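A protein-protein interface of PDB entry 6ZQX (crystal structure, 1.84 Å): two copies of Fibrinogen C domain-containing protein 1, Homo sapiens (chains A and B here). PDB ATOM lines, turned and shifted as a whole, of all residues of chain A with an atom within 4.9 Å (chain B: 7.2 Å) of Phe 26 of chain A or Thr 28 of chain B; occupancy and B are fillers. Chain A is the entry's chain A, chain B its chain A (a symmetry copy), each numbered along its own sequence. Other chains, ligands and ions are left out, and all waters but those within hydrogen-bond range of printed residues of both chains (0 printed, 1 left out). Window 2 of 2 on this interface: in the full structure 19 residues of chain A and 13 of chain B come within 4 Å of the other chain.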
ATOM      1  N   SER A   4     -24.029  -1.182  17.532  1.00  0.00           N
ATOM      2  CA  SER A   4     -24.464  -0.513  18.790  1.00  0.00           C
ATOM      3  C   SER A   4     -24.027   0.964  18.825  1.00  0.00           C
ATOM      4  O   SER A   4     -24.674   1.717  19.591  1.00  0.00           O
ATOM      5  CB  SER A   4     -23.965  -1.258  20.006  1.00  0.00           C
ATOM      6  OG  SER A   4     -22.543  -1.269  20.051  1.00  0.00           O
ATOM      7  N   ARG A   5     -22.993   1.366  18.061  1.00  0.00           N
ATOM      8  CA  ARG A   5     -22.515   2.777  17.972  1.00  0.00           C
ATOM      9  C   ARG A   5     -22.426   3.232  16.516  1.00  0.00           C
ATOM     10  O   ARG A   5     -21.353   3.536  15.997  1.00  0.00           O
ATOM     11  CB  ARG A   5     -21.181   2.938  18.694  1.00  0.00           C
ATOM     12  CG  ARG A   5     -21.312   2.901  20.212  1.00  0.00           C
ATOM     13  CD  ARG A   5     -19.931   3.064  20.823  1.00  0.00           C
ATOM     14  NE  ARG A   5     -19.440   4.439  20.744  1.00  0.00           N
ATOM     15  CZ  ARG A   5     -19.782   5.428  21.577  1.00  0.00           C
ATOM     16  NH1 ARG A   5     -20.648   5.197  22.551  1.00  0.00           N
ATOM     17  NH2 ARG A   5     -19.267   6.642  21.424  1.00  0.00           N
ATOM     18  N   PRO A   6     -23.575   3.370  15.833  1.00  0.00           N
ATOM     19  CA  PRO A   6     -23.600   3.928  14.481  1.00  0.00           C
ATOM     20  C   PRO A   6     -23.163   5.396  14.518  1.00  0.00           C
ATOM     21  O   PRO A   6     -23.521   6.107  15.459  1.00  0.00           O
ATOM     22  CB  PRO A   6     -25.066   3.781  14.051  1.00  0.00           C
ATOM     23  CG  PRO A   6     -25.839   3.758  15.362  1.00  0.00           C
ATOM     24  CD  PRO A   6     -24.920   3.058  16.340  1.00  0.00           C
ATOM     25  N   ARG A   7     -22.424   5.821  13.497  1.00  0.00           N
ATOM     26  CA  ARG A   7     -21.837   7.177  13.433  1.00  0.00           C
ATOM     27  C   ARG A   7     -22.834   8.140  12.792  1.00  0.00           C
ATOM     28  O   ARG A   7     -22.604   9.355  12.888  1.00  0.00           O
ATOM     29  CB  ARG A   7     -20.508   7.152  12.674  1.00  0.00           C
ATOM     30  CG  ARG A   7     -20.668   7.146  11.164  1.00  0.00           C
ATOM     31  CD  ARG A   7     -19.376   6.940  10.387  1.00  0.00           C
ATOM     32  NE  ARG A   7     -19.628   6.808   8.948  1.00  0.00           N
ATOM     33  CZ  ARG A   7     -18.679   6.629   8.031  1.00  0.00           C
ATOM     34  NH1 ARG A   7     -17.406   6.586   8.397  1.00  0.00           N
ATOM     35  NH2 ARG A   7     -18.996   6.516   6.751  1.00  0.00           N
ATOM     36  N   SER A  24     -30.201   7.255  17.972  1.00  0.00           N
ATOM     37  CA  SER A  24     -28.906   7.657  18.566  1.00  0.00           C
ATOM     38  C   SER A  24     -27.803   7.410  17.551  1.00  0.00           C
ATOM     39  O   SER A  24     -27.756   6.294  16.951  1.00  0.00           O
ATOM     40  CB  SER A  24     -28.659   6.903  19.838  1.00  0.00           C
ATOM     41  OG  SER A  24     -29.587   7.299  20.829  1.00  0.00           O
ATOM     42  N   VAL A  25     -26.927   8.401  17.386  1.00  0.00           N
ATOM     43  CA  VAL A  25     -25.706   8.300  16.551  1.00  0.00           C
ATOM     44  C   VAL A  25     -24.527   8.837  17.368  1.00  0.00           C
ATOM     45  O   VAL A  25     -24.751   9.593  18.325  1.00  0.00           O
ATOM     46  CB  VAL A  25     -25.878   9.038  15.213  1.00  0.00           C
ATOM     47  CG1 VAL A  25     -27.041   8.440  14.425  1.00  0.00           C
ATOM     48  CG2 VAL A  25     -26.051  10.527  15.429  1.00  0.00           C
ATOM     49  N   PHE A  26     -23.322   8.437  16.999  1.00  0.00           N
ATOM     50  CA  PHE A  26     -22.114   8.668  17.827  1.00  0.00           C
ATOM     51  C   PHE A  26     -20.963   9.050  16.915  1.00  0.00           C
ATOM     52  O   PHE A  26     -20.159   8.190  16.550  1.00  0.00           O
ATOM     53  CB  PHE A  26     -21.818   7.416  18.651  1.00  0.00           C
ATOM     54  CG  PHE A  26     -22.955   6.932  19.508  1.00  0.00           C
ATOM     55  CD1 PHE A  26     -23.952   6.134  18.973  1.00  0.00           C
ATOM     56  CD2 PHE A  26     -23.042   7.293  20.840  1.00  0.00           C
ATOM     57  CE1 PHE A  26     -24.996   5.675  19.755  1.00  0.00           C
ATOM     58  CE2 PHE A  26     -24.098   6.846  21.624  1.00  0.00           C
ATOM     59  CZ  PHE A  26     -25.079   6.049  21.083  1.00  0.00           C
ATOM     60  N   PRO A  27     -20.866  10.335  16.505  1.00  0.00           N
ATOM     61  CA  PRO A  27     -19.780  10.786  15.644  1.00  0.00           C
ATOM     62  C   PRO A  27     -18.404  10.578  16.301  1.00  0.00           C
ATOM     63  O   PRO A  27     -18.298  10.542  17.513  1.00  0.00           O
ATOM     64  CB  PRO A  27     -20.107  12.266  15.397  1.00  0.00           C
ATOM     65  CG  PRO A  27     -21.606  12.335  15.605  1.00  0.00           C
ATOM     66  CD  PRO A  27     -21.831  11.409  16.784  1.00  0.00           C
ATOM     67  N   THR A  28     -17.381  10.436  15.473  1.00  0.00           N
ATOM     68  CA  THR A  28     -15.984  10.132  15.886  1.00  0.00           C
ATOM     69  C   THR A  28     -15.546  11.057  17.033  1.00  0.00           C
ATOM     70  O   THR A  28     -14.997  10.554  18.040  1.00  0.00           O
ATOM     71  CB  THR A  28     -15.049  10.262  14.683  1.00  0.00           C
ATOM     72  OG1 THR A  28     -15.427   9.222  13.779  1.00  0.00           O
ATOM     73  CG2 THR A  28     -13.585  10.135  15.042  1.00  0.00           C
ATOM     74  N   TYR A  30     -17.535  13.197  18.844  1.00  0.00           N
ATOM     75  CA  TYR A  30     -18.668  13.540  19.736  1.00  0.00           C
ATOM     76  C   TYR A  30     -19.144  12.218  20.343  1.00  0.00           C
ATOM     77  O   TYR A  30     -20.248  11.751  20.055  1.00  0.00           O
ATOM     78  CB  TYR A  30     -19.705  14.296  18.905  1.00  0.00           C
ATOM     79  CG  TYR A  30     -20.650  15.222  19.632  1.00  0.00           C
ATOM     80  CD1 TYR A  30     -21.410  14.813  20.721  1.00  0.00           C
ATOM     81  CD2 TYR A  30     -20.859  16.501  19.144  1.00  0.00           C
ATOM     82  CE1 TYR A  30     -22.306  15.674  21.341  1.00  0.00           C
ATOM     83  CE2 TYR A  30     -21.748  17.373  19.746  1.00  0.00           C
ATOM     84  CZ  TYR A  30     -22.475  16.960  20.846  1.00  0.00           C
ATOM     85  OH  TYR A  30     -23.342  17.864  21.400  1.00  0.00           O
ATOM     86  N   PRO A  31     -18.275  11.508  21.099  1.00  0.00           N
ATOM     87  CA  PRO A  31     -18.560  10.135  21.525  1.00  0.00           C
ATOM     88  C   PRO A  31     -19.743   9.993  22.495  1.00  0.00           C
ATOM     89  O   PRO A  31     -20.304   8.909  22.560  1.00  0.00           O
ATOM     90  CB  PRO A  31     -17.250   9.686  22.203  1.00  0.00           C
ATOM     91  CG  PRO A  31     -16.632  10.975  22.669  1.00  0.00           C
ATOM     92  CD  PRO A  31     -16.946  11.953  21.548  1.00  0.00           C
ATOM     93  N   ALA A  32     -20.146  11.069  23.161  1.00  0.00           N
ATOM     94  CA  ALA A  32     -21.386  11.098  23.971  1.00  0.00           C
ATOM     95  C   ALA A  32     -22.582  10.759  23.059  1.00  0.00           C
ATOM     96  O   ALA A  32     -23.565  10.157  23.537  1.00  0.00           O
ATOM     97  CB  ALA A  32     -21.529  12.444  24.636  1.00  0.00           C
ATOM     98  N   GLY A  33     -22.487  11.143  21.780  1.00  0.00           N
ATOM     99  CA  GLY A  33     -23.550  10.976  20.789  1.00  0.00           C
ATOM    100  C   GLY A  33     -24.740  11.871  21.053  1.00  0.00           C
ATOM    101  O   GLY A  33     -24.747  12.681  22.029  1.00  0.00           O
ATOM    102  N   GLN A  91     -16.262  13.575   9.809  1.00  0.00           N
ATOM    103  CA  GLN A  91     -15.883  12.187  10.181  1.00  0.00           C
ATOM    104  C   GLN A  91     -15.834  11.315   8.920  1.00  0.00           C
ATOM    105  O   GLN A  91     -15.276  10.214   8.997  1.00  0.00           O
ATOM    106  CB  GLN A  91     -16.818  11.637  11.256  1.00  0.00           C
ATOM    107  CG  GLN A  91     -18.133  11.121  10.723  1.00  0.00           C
ATOM    108  CD  GLN A  91     -19.059  10.635  11.805  1.00  0.00           C
ATOM    109  OE1 GLN A  91     -18.628  10.097  12.825  1.00  0.00           O
ATOM    110  NE2 GLN A  91     -20.362  10.761  11.558  1.00  0.00           N
ATOM    111  N   ARG B   5     -21.442  -1.628  33.188  1.00  0.00           N
ATOM    112  CA  ARG B   5     -22.022  -0.319  32.765  1.00  0.00           C
ATOM    113  C   ARG B   5     -23.541  -0.413  32.632  1.00  0.00           C
ATOM    114  O   ARG B   5     -24.108  -0.259  31.551  1.00  0.00           O
ATOM    115  CB  ARG B   5     -21.373   0.162  31.471  1.00  0.00           C
ATOM    116  CG  ARG B   5     -19.948   0.666  31.665  1.00  0.00           C
ATOM    117  CD  ARG B   5     -19.402   1.111  30.320  1.00  0.00           C
ATOM    118  NE  ARG B   5     -19.959   2.391  29.882  1.00  0.00           N
ATOM    119  CZ  ARG B   5     -19.549   3.592  30.300  1.00  0.00           C
ATOM    120  NH1 ARG B   5     -18.579   3.681  31.197  1.00  0.00           N
ATOM    121  NH2 ARG B   5     -20.116   4.697  29.830  1.00  0.00           N
ATOM    122  N   ARG B   7     -27.291   0.915  32.607  1.00  0.00           N
ATOM    123  CA  ARG B   7     -27.824   2.187  32.074  1.00  0.00           C
ATOM    124  C   ARG B   7     -28.794   2.800  33.081  1.00  0.00           C
ATOM    125  O   ARG B   7     -29.137   3.979  32.905  1.00  0.00           O
ATOM    126  CB  ARG B   7     -28.489   1.962  30.714  1.00  0.00           C
ATOM    127  CG  ARG B   7     -29.899   1.406  30.808  1.00  0.00           C
ATOM    128  CD  ARG B   7     -30.516   1.005  29.477  1.00  0.00           C
ATOM    129  NE  ARG B   7     -31.817   0.351  29.661  1.00  0.00           N
ATOM    130  CZ  ARG B   7     -32.583  -0.094  28.666  1.00  0.00           C
ATOM    131  NH1 ARG B   7     -32.194   0.066  27.410  1.00  0.00           N
ATOM    132  NH2 ARG B   7     -33.743  -0.676  28.924  1.00  0.00           N
ATOM    133  N   PHE B  26     -24.992   4.562  33.761  1.00  0.00           N
ATOM    134  CA  PHE B  26     -24.272   5.139  32.600  1.00  0.00           C
ATOM    135  C   PHE B  26     -25.231   5.230  31.428  1.00  0.00           C
ATOM    136  O   PHE B  26     -25.241   4.340  30.574  1.00  0.00           O
ATOM    137  CB  PHE B  26     -23.045   4.285  32.289  1.00  0.00           C
ATOM    138  CG  PHE B  26     -22.101   4.080  33.441  1.00  0.00           C
ATOM    139  CD1 PHE B  26     -22.337   3.091  34.380  1.00  0.00           C
ATOM    140  CD2 PHE B  26     -20.991   4.890  33.600  1.00  0.00           C
ATOM    141  CE1 PHE B  26     -21.469   2.888  35.437  1.00  0.00           C
ATOM    142  CE2 PHE B  26     -20.126   4.698  34.669  1.00  0.00           C
ATOM    143  CZ  PHE B  26     -20.368   3.709  35.593  1.00  0.00           C
ATOM    144  N   PRO B  27     -26.075   6.285  31.366  1.00  0.00           N
ATOM    145  CA  PRO B  27     -27.013   6.454  30.264  1.00  0.00           C
ATOM    146  C   PRO B  27     -26.291   6.571  28.910  1.00  0.00           C
ATOM    147  O   PRO B  27     -25.145   6.978  28.855  1.00  0.00           O
ATOM    148  CB  PRO B  27     -27.786   7.727  30.640  1.00  0.00           C
ATOM    149  CG  PRO B  27     -27.654   7.785  32.148  1.00  0.00           C
ATOM    150  CD  PRO B  27     -26.227   7.334  32.386  1.00  0.00           C
ATOM    151  N   THR B  28     -26.986   6.196  27.847  1.00  0.00           N
ATOM    152  CA  THR B  28     -26.456   6.136  26.458  1.00  0.00           C
ATOM    153  C   THR B  28     -25.709   7.433  26.108  1.00  0.00           C
ATOM    154  O   THR B  28     -24.575   7.356  25.583  1.00  0.00           O
ATOM    155  CB  THR B  28     -27.600   5.876  25.478  1.00  0.00           C
ATOM    156  OG1 THR B  28     -28.077   4.561  25.774  1.00  0.00           O
ATOM    157  CG2 THR B  28     -27.183   5.965  24.027  1.00  0.00           C
ATOM    158  N   HIS B  29     -26.305   8.594  26.362  1.00  0.00           N
ATOM    159  CA  HIS B  29     -25.717   9.897  25.957  1.00  0.00           C
ATOM    160  C   HIS B  29     -25.143  10.655  27.160  1.00  0.00           C
ATOM    161  O   HIS B  29     -24.933  11.863  27.041  1.00  0.00           O
ATOM    162  CB  HIS B  29     -26.760  10.694  25.191  1.00  0.00           C
ATOM    163  CG  HIS B  29     -27.172  10.022  23.934  1.00  0.00           C
ATOM    164  ND1 HIS B  29     -26.261   9.714  22.949  1.00  0.00           N
ATOM    165  CD2 HIS B  29     -28.389   9.622  23.492  1.00  0.00           C
ATOM    166  CE1 HIS B  29     -26.906   9.163  21.929  1.00  0.00           C
ATOM    167  NE2 HIS B  29     -28.214   9.092  22.237  1.00  0.00           N
ATOM    168  N   TYR B  30     -24.843   9.971  28.259  1.00  0.00           N
ATOM    169  CA  TYR B  30     -24.164  10.550  29.443  1.00  0.00           C
ATOM    170  C   TYR B  30     -23.133   9.510  29.890  1.00  0.00           C
ATOM    171  O   TYR B  30     -23.260   8.912  30.960  1.00  0.00           O
ATOM    172  CB  TYR B  30     -25.237  10.900  30.473  1.00  0.00           C
ATOM    173  CG  TYR B  30     -24.918  11.973  31.486  1.00  0.00           C
ATOM    174  CD1 TYR B  30     -23.774  11.942  32.275  1.00  0.00           C
ATOM    175  CD2 TYR B  30     -25.840  12.978  31.726  1.00  0.00           C
ATOM    176  CE1 TYR B  30     -23.529  12.919  33.231  1.00  0.00           C
ATOM    177  CE2 TYR B  30     -25.615  13.959  32.675  1.00  0.00           C
ATOM    178  CZ  TYR B  30     -24.459  13.931  33.431  1.00  0.00           C
ATOM    179  OH  TYR B  30     -24.291  14.925  34.357  1.00  0.00           O
ATOM    180  N   PRO B  31     -22.150   9.167  29.025  1.00  0.00           N
ATOM    181  CA  PRO B  31     -21.264   8.026  29.272  1.00  0.00           C
ATOM    182  C   PRO B  31     -20.339   8.178  30.489  1.00  0.00           C
ATOM    183  O   PRO B  31     -19.901   7.161  31.007  1.00  0.00           O
ATOM    184  CB  PRO B  31     -20.438   7.921  27.975  1.00  0.00           C
ATOM    185  CG  PRO B  31     -20.453   9.323  27.431  1.00  0.00           C
ATOM    186  CD  PRO B  31     -21.858   9.815  27.736  1.00  0.00           C
ATOM    187  N   ALA B  87     -31.368  12.344  30.174  1.00  0.00           N
ATOM    188  CA  ALA B  87     -30.423  11.299  29.708  1.00  0.00           C
ATOM    189  C   ALA B  87     -31.021   9.916  29.989  1.00  0.00           C
ATOM    190  O   ALA B  87     -30.867   9.018  29.152  1.00  0.00           O
ATOM    191  CB  ALA B  87     -29.081  11.460  30.366  1.00  0.00           C
ATOM    192  N   LEU B  88     -31.699   9.747  31.125  1.00  0.00           N
ATOM    193  CA  LEU B  88     -32.311   8.446  31.473  1.00  0.00           C
ATOM    194  C   LEU B  88     -33.526   8.185  30.572  1.00  0.00           C
ATOM    195  O   LEU B  88     -33.582   7.082  29.971  1.00  0.00           O
ATOM    196  CB  LEU B  88     -32.688   8.455  32.952  1.00  0.00           C
ATOM    197  CG  LEU B  88     -31.500   8.358  33.894  1.00  0.00           C
ATOM    198  CD1 LEU B  88     -31.882   8.783  35.284  1.00  0.00           C
ATOM    199  CD2 LEU B  88     -30.889   6.962  33.889  1.00  0.00           C
ATOM    200  N   THR B  90     -34.721   9.330  27.686  1.00  0.00           N
ATOM    201  CA  THR B  90     -34.576   9.284  26.207  1.00  0.00           C
ATOM    202  C   THR B  90     -33.901   7.993  25.731  1.00  0.00           C
ATOM    203  O   THR B  90     -33.836   7.809  24.510  1.00  0.00           O
ATOM    204  CB  THR B  90     -33.815  10.499  25.657  1.00  0.00           C
ATOM    205  OG1 THR B  90     -32.546  10.645  26.294  1.00  0.00           O
ATOM    206  CG2 THR B  90     -34.590  11.781  25.829  1.00  0.00           C
ATOM    207  N   GLN B  91     -33.371   7.147  26.616  1.00  0.00           N
ATOM    208  CA  GLN B  91     -32.513   6.007  26.196  1.00  0.00           C
ATOM    209  C   GLN B  91     -33.373   4.745  26.057  1.00  0.00           C
ATOM    210  O   GLN B  91     -32.890   3.777  25.458  1.00  0.00           O
ATOM    211  CB  GLN B  91     -31.336   5.831  27.154  1.00  0.00           C
ATOM    212  CG  GLN B  91     -31.680   5.088  28.421  1.00  0.00           C
ATOM    213  CD  GLN B  91     -30.519   4.974  29.373  1.00  0.00           C
ATOM    214  OE1 GLN B  91     -29.363   4.862  28.964  1.00  0.00           O
ATOM    215  NE2 GLN B  91     -30.828   4.932  30.668  1.00  0.00           N
ATOM    216  N   ALA B  92     -34.610   4.782  26.563  1.00  0.00           N
ATOM    217  CA  ALA B  92     -35.613   3.694  26.493  1.00  0.00           C
ATOM    218  C   ALA B  92     -36.978   4.275  26.879  1.00  0.00           C
ATOM    219  O   ALA B  92     -37.040   5.474  27.240  1.00  0.00           O
ATOM    220  CB  ALA B  92     -35.216   2.558  27.407  1.00  0.00           C
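The backbone carbonyl oxygen (O) of Ala 32 of chain A is in hydrogen-bond range of a ring nitrogen (ND1) of His 29 of chain B (2.8 Å).
O of Gly 33 of chain A lies close to ND1 of His 29 of chain B, 3.5 Å away.
The side-chain hydroxyl of Ser 24 of chain A sits at hydrogen-bond distance from a ring nitrogen (NE2) of His 29 of chain B.
The side-chain amide oxygen (OE1) of Gln 91 of chain B lies within hydrogen-bond range of the backbone NH (N) of Thr 28 of chain B (2.9 Å).
The backbone carbonyl oxygen (O) of Pro 6 of chain A is in hydrogen-bond range of the backbone NH (N) of Phe 26 of chain A (2.8 Å).
NH2 of Arg 5 of chain B is in hydrogen-bond range of O of Pro 31 of chain B, at 2.7 Å.
CG2 of Thr 28 of chain B touches CZ of Phe 26 of chain A (3.6 Å).
Phe 26 of chain A touches His 29 of chain B.
Ala 32 of chain A touches Thr 28 of chain B (O to O, 3.6 Å).
Pro 31 of chain B touches Ala 32 of chain A.
Printed residues of chain B within 4 Å of Ser 24 of chain A: His 29.
Of the printed residues of chain B, Phe 26 of chain A touches Thr 28 and His 29.
Printed residues of chain B within 4 Å of Ala 32 of chain A: Thr 28 (3.6 Å), His 29 (2.8 Å) and Pro 31 (3.999 Å).
Of the printed residues of chain B, Gly 33 of chain A touches His 29.
Of the printed residues of chain A, Thr 28 of chain B touches Phe 26 and Ala 32.
Printed residues of chain A within 4 Å of His 29 of chain B: Ser 24 (2.7 Å), Phe 26 (3.7 Å), Ala 32 (2.8 Å) and Gly 33 (3.2 Å).
Of the printed residues of chain A, Pro 31 of chain B touches Ala 32.
Ala 92 of chain B touches none of the printed residues of chain A.
The nearest residue of chain A that does not touch Thr 28 of chain B is Ser 24 of chain A (4.2 Å).
The nearest printed residue of chain A that does not touch His 29 of chain B is Val 25 of chain A (4.2 Å).
Of the 13 printed residues of chain B, 3 touch a printed residue of chain A.
Printed residues of chain B that touch a printed residue of chain A: Thr 28, His 29 and Pro 31.
Among the printed residues, 7 pairs touch across the chains.
Among the printed residues, no Asp or Glu carboxylate lies within 4 Å of a Lys or Arg side-chain nitrogen of the other chain.
Phe 26 of chain A touches Thr 28 of chain B, but with the chains exchanged Thr 28 of chain A does not touch Phe 26 of chain B (17.3 Å).
Positions printed for both chains: 5, 7, 26, 27, 28, 30, 31 and 91.
Of the 7 pairs that touch across the chains among the printed residues, none has its exchanged pair printed and touching as well.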
